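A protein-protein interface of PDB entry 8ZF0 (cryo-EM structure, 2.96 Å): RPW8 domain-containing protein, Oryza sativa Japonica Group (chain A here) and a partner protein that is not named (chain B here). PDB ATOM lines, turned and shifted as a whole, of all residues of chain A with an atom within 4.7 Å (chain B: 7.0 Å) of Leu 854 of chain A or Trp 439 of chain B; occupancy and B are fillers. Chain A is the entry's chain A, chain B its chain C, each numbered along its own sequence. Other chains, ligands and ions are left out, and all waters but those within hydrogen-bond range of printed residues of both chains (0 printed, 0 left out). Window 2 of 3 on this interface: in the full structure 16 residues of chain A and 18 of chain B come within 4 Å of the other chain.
Leu 854 of chain A touches just these residues of chain B: Gln 436 and Trp 439. Of the printed residues of chain B, Trp 856 of chain A touches Gln 436 (2.9 Å) and Tyr 440 (3.6 Å). Cys 433 of chain B touches none of the printed residues of chain A. Of chain A, only Leu 854 (3.6 Å) and Leu 857 (3.7 Å) come within 4 Å of Trp 439 of chain B. Printed residues of chain A within 4 Å of Tyr 440 of chain B: Trp 856 (3.6 Å). Of the printed residues of chain A, Leu 443 of chain B touches Leu 857. Leu 509 of chain B touches none of the printed residues of chain A. The nearest residue of chain B that does not touch Leu 854 of chain A is Ala 435 of chain B (6.8 Å). The nearest printed residue of chain A that does not touch Leu 443 of chain B is Trp 856 of chain A (5.1 Å).
O of Asn 853 of chain A is in hydrogen-bond range of NE2 of Gln 436 of chain B (3.1 Å). NE1 of Trp 856 of chain A sits at hydrogen-bond distance from OE1 of Gln 436 of chain B, 2.9 Å away.
Hydrophobic or aromatic side chains of chain A within 4 Å of the printed part of chain B: Leu 854, Trp 856 and Leu 857. Printed residues of chain B that touch a printed residue of chain A: Gln 436, Trp 439, Tyr 440 and Leu 443. Among the printed residues, 7 pairs touch across the chains. Among the printed residues, no Asp or Glu carboxylate lies within 4 Å of a Lys or Arg side-chain nitrogen of the other chain.
The side-chain amide oxygen (OD1) of Asn 853 of chain A sits close to the backbone NH (N) of Asp 855 of chain A, at 3.3 Å. O of Asn 853 of chain A lies within hydrogen-bond range of NE1 of Trp 856 of chain A, 3.4 Å away.
Among the printed residues, pairs that only touch across the chains: Leu 854 of chain A with Gln 436 of chain B, Leu 857 of chain A with Leu 443 of chain B, Leu 854 of chain A with Trp 439 of chain B, Trp 856 of chain A with Tyr 440 of chain B and Leu 857 of chain A with Trp 439 of chain B.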
ATOM      1  N   ASN A 853      -1.321  -1.451 -35.870  1.00  0.00           N
ATOM      2  CA  ASN A 853      -2.736  -1.574 -36.311  1.00  0.00           C
ATOM      3  C   ASN A 853      -3.373  -2.782 -35.623  1.00  0.00           C
ATOM      4  O   ASN A 853      -2.632  -3.559 -34.999  1.00  0.00           O
ATOM      5  CB  ASN A 853      -2.848  -1.730 -37.825  1.00  0.00           C
ATOM      6  CG  ASN A 853      -2.131  -2.954 -38.351  1.00  0.00           C
ATOM      7  OD1 ASN A 853      -2.763  -3.878 -38.856  1.00  0.00           O
ATOM      8  ND2 ASN A 853      -0.814  -2.980 -38.231  1.00  0.00           N
ATOM      9  N   LEU A 854      -4.693  -2.935 -35.741  1.00  0.00           N
ATOM     10  CA  LEU A 854      -5.406  -4.064 -35.088  1.00  0.00           C
ATOM     11  C   LEU A 854      -6.053  -4.940 -36.163  1.00  0.00           C
ATOM     12  O   LEU A 854      -7.122  -5.509 -35.891  1.00  0.00           O
ATOM     13  CB  LEU A 854      -6.474  -3.514 -34.141  1.00  0.00           C
ATOM     14  CG  LEU A 854      -5.983  -3.075 -32.766  1.00  0.00           C
ATOM     15  CD1 LEU A 854      -7.159  -2.675 -31.894  1.00  0.00           C
ATOM     16  CD2 LEU A 854      -5.190  -4.186 -32.101  1.00  0.00           C
ATOM     17  N   ASP A 855      -5.428  -5.033 -37.336  1.00  0.00           N
ATOM     18  CA  ASP A 855      -5.966  -5.884 -38.429  1.00  0.00           C
ATOM     19  C   ASP A 855      -5.716  -7.360 -38.105  1.00  0.00           C
ATOM     20  O   ASP A 855      -6.517  -8.197 -38.545  1.00  0.00           O
ATOM     21  CB  ASP A 855      -5.366  -5.497 -39.778  1.00  0.00           C
ATOM     22  CG  ASP A 855      -5.557  -4.030 -40.115  1.00  0.00           C
ATOM     23  OD1 ASP A 855      -6.154  -3.315 -39.289  1.00  0.00           O
ATOM     24  OD2 ASP A 855      -5.102  -3.612 -41.197  1.00  0.00           O
ATOM     25  N   TRP A 856      -4.649  -7.663 -37.367  1.00  0.00           N
ATOM     26  CA  TRP A 856      -4.312  -9.079 -37.070  1.00  0.00           C
ATOM     27  C   TRP A 856      -5.529  -9.774 -36.454  1.00  0.00           C
ATOM     28  O   TRP A 856      -5.729 -10.964 -36.740  1.00  0.00           O
ATOM     29  CB  TRP A 856      -3.080  -9.166 -36.166  1.00  0.00           C
ATOM     30  CG  TRP A 856      -3.149  -8.340 -34.920  1.00  0.00           C
ATOM     31  CD1 TRP A 856      -3.229  -6.981 -34.832  1.00  0.00           C
ATOM     32  CD2 TRP A 856      -3.134  -8.829 -33.569  1.00  0.00           C
ATOM     33  NE1 TRP A 856      -3.270  -6.593 -33.522  1.00  0.00           N
ATOM     34  CE2 TRP A 856      -3.215  -7.704 -32.724  1.00  0.00           C
ATOM     35  CE3 TRP A 856      -3.063 -10.101 -32.995  1.00  0.00           C
ATOM     36  CZ2 TRP A 856      -3.227  -7.817 -31.336  1.00  0.00           C
ATOM     37  CZ3 TRP A 856      -3.075 -10.213 -31.624  1.00  0.00           C
ATOM     38  CH2 TRP A 856      -3.156  -9.085 -30.809  1.00  0.00           C
ATOM     39  N   LEU A 857      -6.307  -9.055 -35.646  1.00  0.00           N
ATOM     40  CA  LEU A 857      -7.513  -9.634 -34.998  1.00  0.00           C
ATOM     41  C   LEU A 857      -8.628  -9.796 -36.029  1.00  0.00           C
ATOM     42  O   LEU A 857      -9.384 -10.773 -35.917  1.00  0.00           O
ATOM     43  CB  LEU A 857      -7.972  -8.685 -33.889  1.00  0.00           C
ATOM     44  CG  LEU A 857      -6.932  -8.366 -32.818  1.00  0.00           C
ATOM     45  CD1 LEU A 857      -7.507  -7.413 -31.784  1.00  0.00           C
ATOM     46  CD2 LEU A 857      -6.452  -9.639 -32.149  1.00  0.00           C
ATOM     47  N   VAL A 858      -8.729  -8.876 -36.990  1.00  0.00           N
ATOM     48  CA  VAL A 858      -9.864  -8.900 -37.964  1.00  0.00           C
ATOM     49  C   VAL A 858     -10.102 -10.328 -38.451  1.00  0.00           C
ATOM     50  O   VAL A 858     -11.206 -10.847 -38.208  1.00  0.00           O
ATOM     51  CB  VAL A 858      -9.604  -7.960 -39.156  1.00  0.00           C
ATOM     52  CG1 VAL A 858     -10.630  -8.152 -40.261  1.00  0.00           C
ATOM     53  CG2 VAL A 858      -9.551  -6.506 -38.720  1.00  0.00           C
ATOM     54  N   CYS B 433       3.816  -2.088 -28.254  1.00  0.00           N
ATOM     55  CA  CYS B 433       3.972  -3.534 -28.372  1.00  0.00           C
ATOM     56  C   CYS B 433       3.393  -4.244 -27.152  1.00  0.00           C
ATOM     57  O   CYS B 433       2.701  -5.263 -27.281  1.00  0.00           O
ATOM     58  CB  CYS B 433       5.446  -3.893 -28.556  1.00  0.00           C
ATOM     59  SG  CYS B 433       6.247  -3.072 -29.951  1.00  0.00           S
ATOM     60  N   ARG B 434       3.657  -3.710 -25.957  1.00  0.00           N
ATOM     61  CA  ARG B 434       3.060  -4.267 -24.749  1.00  0.00           C
ATOM     62  C   ARG B 434       1.544  -4.113 -24.760  1.00  0.00           C
ATOM     63  O   ARG B 434       0.826  -4.995 -24.276  1.00  0.00           O
ATOM     64  CB  ARG B 434       3.662  -3.596 -23.513  1.00  0.00           C
ATOM     65  CG  ARG B 434       3.059  -4.053 -22.197  1.00  0.00           C
ATOM     66  CD  ARG B 434       3.309  -3.049 -21.088  1.00  0.00           C
ATOM     67  NE  ARG B 434       2.181  -2.143 -20.914  1.00  0.00           N
ATOM     68  CZ  ARG B 434       2.276  -0.913 -20.427  1.00  0.00           C
ATOM     69  NH1 ARG B 434       3.438  -0.409 -20.047  1.00  0.00           N
ATOM     70  NH2 ARG B 434       1.178  -0.173 -20.319  1.00  0.00           N
ATOM     71  N   ALA B 435       1.039  -3.007 -25.312  1.00  0.00           N
ATOM     72  CA  ALA B 435      -0.409  -2.843 -25.436  1.00  0.00           C
ATOM     73  C   ALA B 435      -1.012  -3.911 -26.345  1.00  0.00           C
ATOM     74  O   ALA B 435      -2.080  -4.464 -26.050  1.00  0.00           O
ATOM     75  CB  ALA B 435      -0.736  -1.445 -25.957  1.00  0.00           C
ATOM     76  N   GLN B 436      -0.345  -4.207 -27.462  1.00  0.00           N
ATOM     77  CA  GLN B 436      -0.820  -5.263 -28.353  1.00  0.00           C
ATOM     78  C   GLN B 436      -0.767  -6.625 -27.671  1.00  0.00           C
ATOM     79  O   GLN B 436      -1.656  -7.463 -27.871  1.00  0.00           O
ATOM     80  CB  GLN B 436       0.000  -5.273 -29.643  1.00  0.00           C
ATOM     81  CG  GLN B 436      -0.090  -3.988 -30.447  1.00  0.00           C
ATOM     82  CD  GLN B 436      -0.917  -4.148 -31.707  1.00  0.00           C
ATOM     83  OE1 GLN B 436      -1.966  -4.790 -31.697  1.00  0.00           O
ATOM     84  NE2 GLN B 436      -0.445  -3.562 -32.801  1.00  0.00           N
ATOM     85  N   ILE B 437       0.276  -6.871 -26.875  1.00  0.00           N
ATOM     86  CA  ILE B 437       0.340  -8.112 -26.104  1.00  0.00           C
ATOM     87  C   ILE B 437      -0.826  -8.193 -25.126  1.00  0.00           C
ATOM     88  O   ILE B 437      -1.412  -9.264 -24.916  1.00  0.00           O
ATOM     89  CB  ILE B 437       1.697  -8.227 -25.383  1.00  0.00           C
ATOM     90  CG1 ILE B 437       2.831  -8.350 -26.401  1.00  0.00           C
ATOM     91  CG2 ILE B 437       1.705  -9.418 -24.439  1.00  0.00           C
ATOM     92  CD1 ILE B 437       2.799  -9.639 -27.191  1.00  0.00           C
ATOM     93  N   GLU B 438      -1.180  -7.064 -24.508  1.00  0.00           N
ATOM     94  CA  GLU B 438      -2.327  -7.036 -23.603  1.00  0.00           C
ATOM     95  C   GLU B 438      -3.619  -7.355 -24.348  1.00  0.00           C
ATOM     96  O   GLU B 438      -4.475  -8.086 -23.836  1.00  0.00           O
ATOM     97  CB  GLU B 438      -2.412  -5.670 -22.916  1.00  0.00           C
ATOM     98  CG  GLU B 438      -3.294  -5.611 -21.668  1.00  0.00           C
ATOM     99  CD  GLU B 438      -4.777  -5.712 -21.969  1.00  0.00           C
ATOM    100  OE1 GLU B 438      -5.223  -5.126 -22.978  1.00  0.00           O
ATOM    101  OE2 GLU B 438      -5.498  -6.380 -21.197  1.00  0.00           O
ATOM    102  N   TRP B 439      -3.780  -6.805 -25.554  1.00  0.00           N
ATOM    103  CA  TRP B 439      -4.949  -7.136 -26.367  1.00  0.00           C
ATOM    104  C   TRP B 439      -4.992  -8.625 -26.693  1.00  0.00           C
ATOM    105  O   TRP B 439      -6.053  -9.261 -26.616  1.00  0.00           O
ATOM    106  CB  TRP B 439      -4.950  -6.312 -27.654  1.00  0.00           C
ATOM    107  CG  TRP B 439      -5.579  -4.961 -27.519  1.00  0.00           C
ATOM    108  CD1 TRP B 439      -5.087  -3.892 -26.831  1.00  0.00           C
ATOM    109  CD2 TRP B 439      -6.817  -4.533 -28.095  1.00  0.00           C
ATOM    110  NE1 TRP B 439      -5.945  -2.824 -26.940  1.00  0.00           N
ATOM    111  CE2 TRP B 439      -7.015  -3.192 -27.712  1.00  0.00           C
ATOM    112  CE3 TRP B 439      -7.780  -5.153 -28.898  1.00  0.00           C
ATOM    113  CZ2 TRP B 439      -8.135  -2.462 -28.102  1.00  0.00           C
ATOM    114  CZ3 TRP B 439      -8.891  -4.426 -29.284  1.00  0.00           C
ATOM    115  CH2 TRP B 439      -9.059  -3.096 -28.887  1.00  0.00           C
ATOM    116  N   TYR B 440      -3.842  -9.198 -27.055  1.00  0.00           N
ATOM    117  CA  TYR B 440      -3.779 -10.626 -27.347  1.00  0.00           C
ATOM    118  C   TYR B 440      -4.166 -11.454 -26.129  1.00  0.00           C
ATOM    119  O   TYR B 440      -4.887 -12.452 -26.249  1.00  0.00           O
ATOM    120  CB  TYR B 440      -2.377 -11.001 -27.827  1.00  0.00           C
ATOM    121  CG  TYR B 440      -2.154 -12.488 -27.977  1.00  0.00           C
ATOM    122  CD1 TYR B 440      -2.744 -13.199 -29.014  1.00  0.00           C
ATOM    123  CD2 TYR B 440      -1.353 -13.183 -27.081  1.00  0.00           C
ATOM    124  CE1 TYR B 440      -2.542 -14.559 -29.152  1.00  0.00           C
ATOM    125  CE2 TYR B 440      -1.145 -14.541 -27.212  1.00  0.00           C
ATOM    126  CZ  TYR B 440      -1.742 -15.225 -28.248  1.00  0.00           C
ATOM    127  OH  TYR B 440      -1.537 -16.578 -28.382  1.00  0.00           O
ATOM    128  N   LYS B 441      -3.687 -11.060 -24.947  1.00  0.00           N
ATOM    129  CA  LYS B 441      -4.053 -11.769 -23.724  1.00  0.00           C
ATOM    130  C   LYS B 441      -5.550 -11.674 -23.459  1.00  0.00           C
ATOM    131  O   LYS B 441      -6.198 -12.670 -23.119  1.00  0.00           O
ATOM    132  CB  LYS B 441      -3.267 -11.215 -22.536  1.00  0.00           C
ATOM    133  CG  LYS B 441      -3.787 -11.702 -21.195  1.00  0.00           C
ATOM    134  CD  LYS B 441      -3.309 -10.829 -20.051  1.00  0.00           C
ATOM    135  CE  LYS B 441      -3.860 -11.329 -18.725  1.00  0.00           C
ATOM    136  NZ  LYS B 441      -5.335 -11.524 -18.776  1.00  0.00           N
ATOM    137  N   ALA B 442      -6.118 -10.475 -23.614  1.00  0.00           N
ATOM    138  CA  ALA B 442      -7.543 -10.294 -23.359  1.00  0.00           C
ATOM    139  C   ALA B 442      -8.395 -11.053 -24.367  1.00  0.00           C
ATOM    140  O   ALA B 442      -9.557 -11.368 -24.085  1.00  0.00           O
ATOM    141  CB  ALA B 442      -7.896  -8.807 -23.377  1.00  0.00           C
ATOM    142  N   LEU B 443      -7.843 -11.340 -25.548  1.00  0.00           N
ATOM    143  CA  LEU B 443      -8.600 -12.080 -26.555  1.00  0.00           C
ATOM    144  C   LEU B 443      -8.958 -13.482 -26.065  1.00  0.00           C
ATOM    145  O   LEU B 443     -10.095 -13.934 -26.236  1.00  0.00           O
ATOM    146  CB  LEU B 443      -7.799 -12.143 -27.858  1.00  0.00           C
ATOM    147  CG  LEU B 443      -8.486 -12.265 -29.227  1.00  0.00           C
ATOM    148  CD1 LEU B 443      -7.438 -12.429 -30.318  1.00  0.00           C
ATOM    149  CD2 LEU B 443      -9.501 -13.399 -29.306  1.00  0.00           C
ATOM    150  N   PHE B 444      -8.007 -14.177 -25.437  1.00  0.00           N
ATOM    151  CA  PHE B 444      -8.176 -15.580 -25.069  1.00  0.00           C
ATOM    152  C   PHE B 444      -8.432 -15.778 -23.578  1.00  0.00           C
ATOM    153  O   PHE B 444      -8.203 -16.875 -23.058  1.00  0.00           O
ATOM    154  CB  PHE B 444      -6.954 -16.394 -25.497  1.00  0.00           C
ATOM    155  CG  PHE B 444      -6.746 -16.453 -26.984  1.00  0.00           C
ATOM    156  CD1 PHE B 444      -6.113 -15.420 -27.653  1.00  0.00           C
ATOM    157  CD2 PHE B 444      -7.178 -17.549 -27.711  1.00  0.00           C
ATOM    158  CE1 PHE B 444      -5.921 -15.476 -29.021  1.00  0.00           C
ATOM    159  CE2 PHE B 444      -6.988 -17.612 -29.077  1.00  0.00           C
ATOM    160  CZ  PHE B 444      -6.359 -16.574 -29.733  1.00  0.00           C
ATOM    161  N   LEU B 509       3.399  -9.265 -17.341  1.00  0.00           N
ATOM    162  CA  LEU B 509       2.599  -9.538 -18.528  1.00  0.00           C
ATOM    163  C   LEU B 509       3.271 -10.500 -19.503  1.00  0.00           C
ATOM    164  O   LEU B 509       2.573 -11.275 -20.167  1.00  0.00           O
ATOM    165  CB  LEU B 509       2.259  -8.230 -19.249  1.00  0.00           C
ATOM    166  CG  LEU B 509       1.447  -8.370 -20.538  1.00  0.00           C
ATOM    167  CD1 LEU B 509       0.037  -8.846 -20.227  1.00  0.00           C
ATOM    168  CD2 LEU B 509       1.410  -7.063 -21.301  1.00  0.00           C
